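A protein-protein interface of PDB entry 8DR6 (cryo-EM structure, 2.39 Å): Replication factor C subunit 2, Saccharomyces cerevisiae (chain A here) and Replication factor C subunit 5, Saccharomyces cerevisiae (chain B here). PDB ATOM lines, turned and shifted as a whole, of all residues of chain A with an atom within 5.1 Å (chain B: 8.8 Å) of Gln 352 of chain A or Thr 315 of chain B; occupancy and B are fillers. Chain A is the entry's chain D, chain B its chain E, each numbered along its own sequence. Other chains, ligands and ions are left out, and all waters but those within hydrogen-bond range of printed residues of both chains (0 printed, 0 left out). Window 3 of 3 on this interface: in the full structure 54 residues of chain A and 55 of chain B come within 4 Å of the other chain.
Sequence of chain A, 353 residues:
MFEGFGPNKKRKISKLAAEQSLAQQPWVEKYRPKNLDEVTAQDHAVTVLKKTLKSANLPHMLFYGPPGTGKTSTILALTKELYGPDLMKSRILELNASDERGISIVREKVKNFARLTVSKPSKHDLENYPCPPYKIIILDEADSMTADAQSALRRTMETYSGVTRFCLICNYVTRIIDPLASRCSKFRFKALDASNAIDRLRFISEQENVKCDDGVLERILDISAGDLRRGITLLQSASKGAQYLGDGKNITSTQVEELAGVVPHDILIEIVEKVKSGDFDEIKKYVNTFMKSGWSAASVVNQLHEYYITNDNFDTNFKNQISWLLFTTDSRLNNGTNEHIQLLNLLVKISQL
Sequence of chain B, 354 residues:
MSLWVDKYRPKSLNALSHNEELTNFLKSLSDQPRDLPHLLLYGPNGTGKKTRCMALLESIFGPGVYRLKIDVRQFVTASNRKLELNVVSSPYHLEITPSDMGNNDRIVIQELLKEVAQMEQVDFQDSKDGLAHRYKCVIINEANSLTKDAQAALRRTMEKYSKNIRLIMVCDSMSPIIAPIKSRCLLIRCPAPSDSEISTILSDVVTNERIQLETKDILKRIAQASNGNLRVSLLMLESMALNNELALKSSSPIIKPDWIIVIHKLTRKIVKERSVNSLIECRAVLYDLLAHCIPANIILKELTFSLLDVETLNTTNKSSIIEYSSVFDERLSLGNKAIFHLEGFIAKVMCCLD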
ATOM      1  N   PHE A 280     -19.305  28.516 -20.828  1.00  0.00           N
ATOM      2  CA  PHE A 280     -18.272  28.802 -21.818  1.00  0.00           C
ATOM      3  C   PHE A 280     -18.418  30.210 -22.384  1.00  0.00           C
ATOM      4  O   PHE A 280     -17.426  30.933 -22.528  1.00  0.00           O
ATOM      5  CB  PHE A 280     -18.323  27.767 -22.942  1.00  0.00           C
ATOM      6  CG  PHE A 280     -17.120  27.789 -23.843  1.00  0.00           C
ATOM      7  CD1 PHE A 280     -16.982  28.762 -24.819  1.00  0.00           C
ATOM      8  CD2 PHE A 280     -16.126  26.832 -23.716  1.00  0.00           C
ATOM      9  CE1 PHE A 280     -15.876  28.783 -25.647  1.00  0.00           C
ATOM     10  CE2 PHE A 280     -15.019  26.848 -24.542  1.00  0.00           C
ATOM     11  CZ  PHE A 280     -14.893  27.825 -25.508  1.00  0.00           C
ATOM     12  N   VAL A 348     -10.979  27.549 -19.597  1.00  0.00           N
ATOM     13  CA  VAL A 348     -12.033  26.597 -19.934  1.00  0.00           C
ATOM     14  C   VAL A 348     -11.724  25.230 -19.336  1.00  0.00           C
ATOM     15  O   VAL A 348     -12.610  24.567 -18.782  1.00  0.00           O
ATOM     16  CB  VAL A 348     -12.209  26.522 -21.462  1.00  0.00           C
ATOM     17  CG1 VAL A 348     -12.983  25.268 -21.852  1.00  0.00           C
ATOM     18  CG2 VAL A 348     -12.907  27.771 -21.975  1.00  0.00           C
ATOM     19  N   LYS A 349     -10.471  24.784 -19.438  1.00  0.00           N
ATOM     20  CA  LYS A 349     -10.105  23.484 -18.887  1.00  0.00           C
ATOM     21  C   LYS A 349     -10.276  23.457 -17.374  1.00  0.00           C
ATOM     22  O   LYS A 349     -10.756  22.462 -16.817  1.00  0.00           O
ATOM     23  CB  LYS A 349      -8.667  23.139 -19.275  1.00  0.00           C
ATOM     24  CG  LYS A 349      -8.540  22.531 -20.663  1.00  0.00           C
ATOM     25  CD  LYS A 349      -7.088  22.374 -21.077  1.00  0.00           C
ATOM     26  CE  LYS A 349      -6.946  21.412 -22.244  1.00  0.00           C
ATOM     27  NZ  LYS A 349      -7.182  19.999 -21.840  1.00  0.00           N
ATOM     28  N   ILE A 350      -9.891  24.536 -16.690  1.00  0.00           N
ATOM     29  CA  ILE A 350     -10.072  24.586 -15.242  1.00  0.00           C
ATOM     30  C   ILE A 350     -11.555  24.566 -14.890  1.00  0.00           C
ATOM     31  O   ILE A 350     -11.969  23.912 -13.926  1.00  0.00           O
ATOM     32  CB  ILE A 350      -9.369  25.822 -14.651  1.00  0.00           C
ATOM     33  CG1 ILE A 350      -7.861  25.756 -14.905  1.00  0.00           C
ATOM     34  CG2 ILE A 350      -9.637  25.920 -13.153  1.00  0.00           C
ATOM     35  CD1 ILE A 350      -7.149  27.074 -14.684  1.00  0.00           C
ATOM     36  N   SER A 351     -12.378  25.280 -15.663  1.00  0.00           N
ATOM     37  CA  SER A 351     -13.801  25.359 -15.351  1.00  0.00           C
ATOM     38  C   SER A 351     -14.479  23.998 -15.440  1.00  0.00           C
ATOM     39  O   SER A 351     -15.529  23.789 -14.822  1.00  0.00           O
ATOM     40  CB  SER A 351     -14.486  26.351 -16.291  1.00  0.00           C
ATOM     41  OG  SER A 351     -14.955  25.704 -17.460  1.00  0.00           O
ATOM     42  N   GLN A 352     -13.904  23.063 -16.197  1.00  0.00           N
ATOM     43  CA  GLN A 352     -14.489  21.745 -16.395  1.00  0.00           C
ATOM     44  C   GLN A 352     -13.849  20.681 -15.509  1.00  0.00           C
ATOM     45  O   GLN A 352     -14.086  19.486 -15.716  1.00  0.00           O
ATOM     46  CB  GLN A 352     -14.381  21.339 -17.867  1.00  0.00           C
ATOM     47  CG  GLN A 352     -15.319  22.107 -18.785  1.00  0.00           C
ATOM     48  CD  GLN A 352     -14.913  22.019 -20.242  1.00  0.00           C
ATOM     49  OE1 GLN A 352     -13.908  21.396 -20.584  1.00  0.00           O
ATOM     50  NE2 GLN A 352     -15.697  22.646 -21.112  1.00  0.00           N
ATOM     51  N   LEU A 353     -13.046  21.086 -14.530  1.00  0.00           N
ATOM     52  CA  LEU A 353     -12.419  20.138 -13.618  1.00  0.00           C
ATOM     53  C   LEU A 353     -13.398  19.711 -12.531  1.00  0.00           C
ATOM     54  O   LEU A 353     -13.250  18.649 -11.926  1.00  0.00           O
ATOM     55  CB  LEU A 353     -11.165  20.747 -12.984  1.00  0.00           C
ATOM     56  CG  LEU A 353      -9.867  20.684 -13.793  1.00  0.00           C
ATOM     57  CD1 LEU A 353      -8.723  21.285 -12.991  1.00  0.00           C
ATOM     58  CD2 LEU A 353      -9.534  19.258 -14.207  1.00  0.00           C
ATOM     59  OXT LEU A 353     -14.360  20.417 -12.232  1.00  0.00           O
ATOM     60  N   LEU B 308     -15.993  29.747 -32.517  1.00  0.00           N
ATOM     61  CA  LEU B 308     -16.541  29.774 -31.168  1.00  0.00           C
ATOM     62  C   LEU B 308     -17.788  30.640 -31.052  1.00  0.00           C
ATOM     63  O   LEU B 308     -18.534  30.493 -30.079  1.00  0.00           O
ATOM     64  CB  LEU B 308     -15.480  30.277 -30.184  1.00  0.00           C
ATOM     65  CG  LEU B 308     -14.300  29.341 -29.907  1.00  0.00           C
ATOM     66  CD1 LEU B 308     -13.281  30.028 -29.012  1.00  0.00           C
ATOM     67  CD2 LEU B 308     -14.762  28.036 -29.280  1.00  0.00           C
ATOM     68  N   VAL B 310     -20.276  30.593 -33.259  1.00  0.00           N
ATOM     69  CA  VAL B 310     -21.402  29.934 -33.910  1.00  0.00           C
ATOM     70  C   VAL B 310     -22.384  29.472 -32.842  1.00  0.00           C
ATOM     71  O   VAL B 310     -21.999  28.833 -31.856  1.00  0.00           O
ATOM     72  CB  VAL B 310     -20.923  28.763 -34.776  1.00  0.00           C
ATOM     73  CG1 VAL B 310     -22.109  28.033 -35.388  1.00  0.00           C
ATOM     74  CG2 VAL B 310     -19.976  29.258 -35.859  1.00  0.00           C
ATOM     75  N   GLU B 311     -23.662  29.793 -33.034  1.00  0.00           N
ATOM     76  CA  GLU B 311     -24.690  29.503 -32.042  1.00  0.00           C
ATOM     77  C   GLU B 311     -25.196  28.068 -32.101  1.00  0.00           C
ATOM     78  O   GLU B 311     -25.898  27.641 -31.178  1.00  0.00           O
ATOM     79  CB  GLU B 311     -25.868  30.466 -32.218  1.00  0.00           C
ATOM     80  CG  GLU B 311     -25.732  31.761 -31.435  1.00  0.00           C
ATOM     81  CD  GLU B 311     -26.397  32.935 -32.128  1.00  0.00           C
ATOM     82  OE1 GLU B 311     -27.378  32.713 -32.868  1.00  0.00           O
ATOM     83  OE2 GLU B 311     -25.939  34.081 -31.931  1.00  0.00           O
ATOM     84  N   THR B 312     -24.864  27.315 -33.149  1.00  0.00           N
ATOM     85  CA  THR B 312     -25.320  25.939 -33.292  1.00  0.00           C
ATOM     86  C   THR B 312     -24.362  24.920 -32.686  1.00  0.00           C
ATOM     87  O   THR B 312     -24.684  23.729 -32.673  1.00  0.00           O
ATOM     88  CB  THR B 312     -25.535  25.603 -34.773  1.00  0.00           C
ATOM     89  OG1 THR B 312     -24.276  25.609 -35.458  1.00  0.00           O
ATOM     90  CG2 THR B 312     -26.469  26.614 -35.424  1.00  0.00           C
ATOM     91  N   LEU B 313     -23.207  25.353 -32.188  1.00  0.00           N
ATOM     92  CA  LEU B 313     -22.234  24.433 -31.616  1.00  0.00           C
ATOM     93  C   LEU B 313     -22.454  24.286 -30.116  1.00  0.00           C
ATOM     94  O   LEU B 313     -22.877  25.227 -29.439  1.00  0.00           O
ATOM     95  CB  LEU B 313     -20.811  24.924 -31.888  1.00  0.00           C
ATOM     96  CG  LEU B 313     -20.419  25.087 -33.359  1.00  0.00           C
ATOM     97  CD1 LEU B 313     -18.935  25.397 -33.481  1.00  0.00           C
ATOM     98  CD2 LEU B 313     -20.775  23.846 -34.164  1.00  0.00           C
ATOM     99  N   ASN B 314     -22.162  23.094 -29.600  1.00  0.00           N
ATOM    100  CA  ASN B 314     -22.310  22.809 -28.182  1.00  0.00           C
ATOM    101  C   ASN B 314     -21.004  23.104 -27.445  1.00  0.00           C
ATOM    102  O   ASN B 314     -19.978  23.439 -28.043  1.00  0.00           O
ATOM    103  CB  ASN B 314     -22.748  21.359 -27.973  1.00  0.00           C
ATOM    104  CG  ASN B 314     -21.760  20.361 -28.541  1.00  0.00           C
ATOM    105  OD1 ASN B 314     -20.605  20.301 -28.118  1.00  0.00           O
ATOM    106  ND2 ASN B 314     -22.210  19.566 -29.505  1.00  0.00           N
ATOM    107  N   THR B 315     -21.043  22.975 -26.116  1.00  0.00           N
ATOM    108  CA  THR B 315     -19.882  23.319 -25.301  1.00  0.00           C
ATOM    109  C   THR B 315     -18.696  22.408 -25.600  1.00  0.00           C
ATOM    110  O   THR B 315     -17.551  22.871 -25.655  1.00  0.00           O
ATOM    111  CB  THR B 315     -20.247  23.248 -23.817  1.00  0.00           C
ATOM    112  OG1 THR B 315     -21.144  24.317 -23.491  1.00  0.00           O
ATOM    113  CG2 THR B 315     -19.001  23.355 -22.948  1.00  0.00           C
ATOM    114  N   THR B 316     -18.948  21.109 -25.783  1.00  0.00           N
ATOM    115  CA  THR B 316     -17.855  20.177 -26.049  1.00  0.00           C
ATOM    116  C   THR B 316     -17.134  20.531 -27.343  1.00  0.00           C
ATOM    117  O   THR B 316     -15.898  20.485 -27.411  1.00  0.00           O
ATOM    118  CB  THR B 316     -18.391  18.747 -26.109  1.00  0.00           C
ATOM    119  OG1 THR B 316     -18.976  18.397 -24.848  1.00  0.00           O
ATOM    120  CG2 THR B 316     -17.272  17.766 -26.434  1.00  0.00           C
ATOM    121  N   ASN B 317     -17.891  20.879 -28.386  1.00  0.00           N
ATOM    122  CA  ASN B 317     -17.273  21.258 -29.651  1.00  0.00           C
ATOM    123  C   ASN B 317     -16.387  22.483 -29.480  1.00  0.00           C
ATOM    124  O   ASN B 317     -15.271  22.530 -30.010  1.00  0.00           O
ATOM    125  CB  ASN B 317     -18.350  21.521 -30.703  1.00  0.00           C
ATOM    126  CG  ASN B 317     -19.159  20.283 -31.033  1.00  0.00           C
ATOM    127  OD1 ASN B 317     -18.718  19.158 -30.799  1.00  0.00           O
ATOM    128  ND2 ASN B 317     -20.349  20.485 -31.585  1.00  0.00           N
ATOM    129  N   LYS B 318     -16.864  23.485 -28.740  1.00  0.00           N
ATOM    130  CA  LYS B 318     -16.072  24.694 -28.535  1.00  0.00           C
ATOM    131  C   LYS B 318     -14.816  24.403 -27.721  1.00  0.00           C
ATOM    132  O   LYS B 318     -13.744  24.951 -28.005  1.00  0.00           O
ATOM    133  CB  LYS B 318     -16.929  25.762 -27.854  1.00  0.00           C
ATOM    134  CG  LYS B 318     -17.788  26.564 -28.825  1.00  0.00           C
ATOM    135  CD  LYS B 318     -19.215  26.730 -28.325  1.00  0.00           C
ATOM    136  CE  LYS B 318     -19.285  27.635 -27.108  1.00  0.00           C
ATOM    137  NZ  LYS B 318     -20.666  27.723 -26.560  1.00  0.00           N
ATOM    138  N   SER B 319     -14.927  23.546 -26.703  1.00  0.00           N
ATOM    139  CA  SER B 319     -13.750  23.180 -25.918  1.00  0.00           C
ATOM    140  C   SER B 319     -12.714  22.470 -26.783  1.00  0.00           C
ATOM    141  O   SER B 319     -11.515  22.779 -26.713  1.00  0.00           O
ATOM    142  CB  SER B 319     -14.161  22.296 -24.742  1.00  0.00           C
ATOM    143  OG  SER B 319     -15.254  22.859 -24.037  1.00  0.00           O
ATOM    144  N   SER B 320     -13.158  21.519 -27.607  1.00  0.00           N
ATOM    145  CA  SER B 320     -12.233  20.842 -28.509  1.00  0.00           C
ATOM    146  C   SER B 320     -11.605  21.827 -29.486  1.00  0.00           C
ATOM    147  O   SER B 320     -10.405  21.748 -29.778  1.00  0.00           O
ATOM    148  CB  SER B 320     -12.957  19.726 -29.261  1.00  0.00           C
ATOM    149  OG  SER B 320     -13.235  18.631 -28.406  1.00  0.00           O
ATOM    150  N   ILE B 321     -12.404  22.765 -29.998  1.00  0.00           N
ATOM    151  CA  ILE B 321     -11.898  23.737 -30.960  1.00  0.00           C
ATOM    152  C   ILE B 321     -10.809  24.590 -30.325  1.00  0.00           C
ATOM    153  O   ILE B 321      -9.757  24.829 -30.926  1.00  0.00           O
ATOM    154  CB  ILE B 321     -13.049  24.602 -31.503  1.00  0.00           C
ATOM    155  CG1 ILE B 321     -13.895  23.798 -32.493  1.00  0.00           C
ATOM    156  CG2 ILE B 321     -12.506  25.862 -32.167  1.00  0.00           C
ATOM    157  CD1 ILE B 321     -15.263  24.392 -32.753  1.00  0.00           C
ATOM    158  N   ILE B 322     -11.043  25.066 -29.100  1.00  0.00           N
ATOM    159  CA  ILE B 322     -10.051  25.924 -28.458  1.00  0.00           C
ATOM    160  C   ILE B 322      -8.793  25.135 -28.105  1.00  0.00           C
ATOM    161  O   ILE B 322      -7.675  25.653 -28.226  1.00  0.00           O
ATOM    162  CB  ILE B 322     -10.656  26.626 -27.224  1.00  0.00           C
ATOM    163  CG1 ILE B 322      -9.689  27.678 -26.667  1.00  0.00           C
ATOM    164  CG2 ILE B 322     -11.026  25.627 -26.144  1.00  0.00           C
ATOM    165  CD1 ILE B 322      -9.345  28.786 -27.641  1.00  0.00           C
ATOM    166  N   GLU B 323      -8.939  23.878 -27.673  1.00  0.00           N
ATOM    167  CA  GLU B 323      -7.753  23.072 -27.392  1.00  0.00           C
ATOM    168  C   GLU B 323      -6.924  22.853 -28.654  1.00  0.00           C
ATOM    169  O   GLU B 323      -5.692  23.005 -28.637  1.00  0.00           O
ATOM    170  CB  GLU B 323      -8.164  21.732 -26.782  1.00  0.00           C
ATOM    171  CG  GLU B 323      -6.992  20.861 -26.357  1.00  0.00           C
ATOM    172  CD  GLU B 323      -7.386  19.789 -25.358  1.00  0.00           C
ATOM    173  OE1 GLU B 323      -6.522  18.961 -25.001  1.00  0.00           O
ATOM    174  OE2 GLU B 323      -8.560  19.772 -24.931  1.00  0.00           O
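Hydrophobic or aromatic side chains of chain B that line the printed part of chain A: Leu 308.
Printed residues of chain A that touch a printed residue of chain B: Phe 280, Val 348, Lys 349 and Gln 352.
Hydrophobic or aromatic side chains of chain A that line the printed part of chain B: Phe 280 and Val 348.
Among the printed residues, 7 pairs touch across the chains.
O of Thr 315 of chain B lies within hydrogen-bond range of OG of Ser 319 of chain B (2.8 Å).
The backbone carbonyl oxygen (O) of Val 348 of chain A sits at hydrogen-bond distance from the side-chain hydroxyl (OG) of Ser 351 of chain A.
Printed residues of chain B within 4 Å of Phe 280 of chain A: Leu 308, Lys 318 and Ser 319.
Printed residues of chain B within 4 Å of Val 348 of chain A: Ser 319 (3.97 Å).
Of the printed residues of chain B, Lys 349 of chain A touches Glu 323.
Gln 352 of chain A touches just these residues of chain B: Thr 315 (3.8 Å) and Ser 319 (3.0 Å).
Thr 312 of chain B touches none of the printed residues of chain A.
Of chain A, only Gln 352 (3.8 Å) comes within 4 Å of Thr 315 of chain B.
Ile 322 of chain B touches none of the printed residues of chain A.
The nearest residue of chain B that does not touch Gln 352 of chain A is Thr 316 of chain B (5.9 Å).
The nearest residue of chain A that does not touch Thr 315 of chain B is Phe 280 of chain A (4.5 Å).
The nearest printed residue of chain A that does not touch Ser 319 of chain B is Lys 349 of chain A (6.5 Å).
CD2 of Leu 308 of chain B touches CZ of Phe 280 of chain A (3.8 Å).
Lys 318 of chain B touches Phe 280 of chain A (CE to CD1, 3.4 Å).
Phe 280 of chain A touches Ser 319 of chain B (CE2 to N, 3.9 Å).
Val 348 of chain A touches Ser 319 of chain B (CG1 to OG, 3.97 Å).
Gln 352 of chain A touches Thr 315 of chain B.
NE2 of Gln 352 of chain A is in hydrogen-bond range of OG of Ser 319 of chain B.
OE1 of Glu 323 of chain B lies within salt-bridge range of NZ of Lys 349 of chain A, at 3.4 Å.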
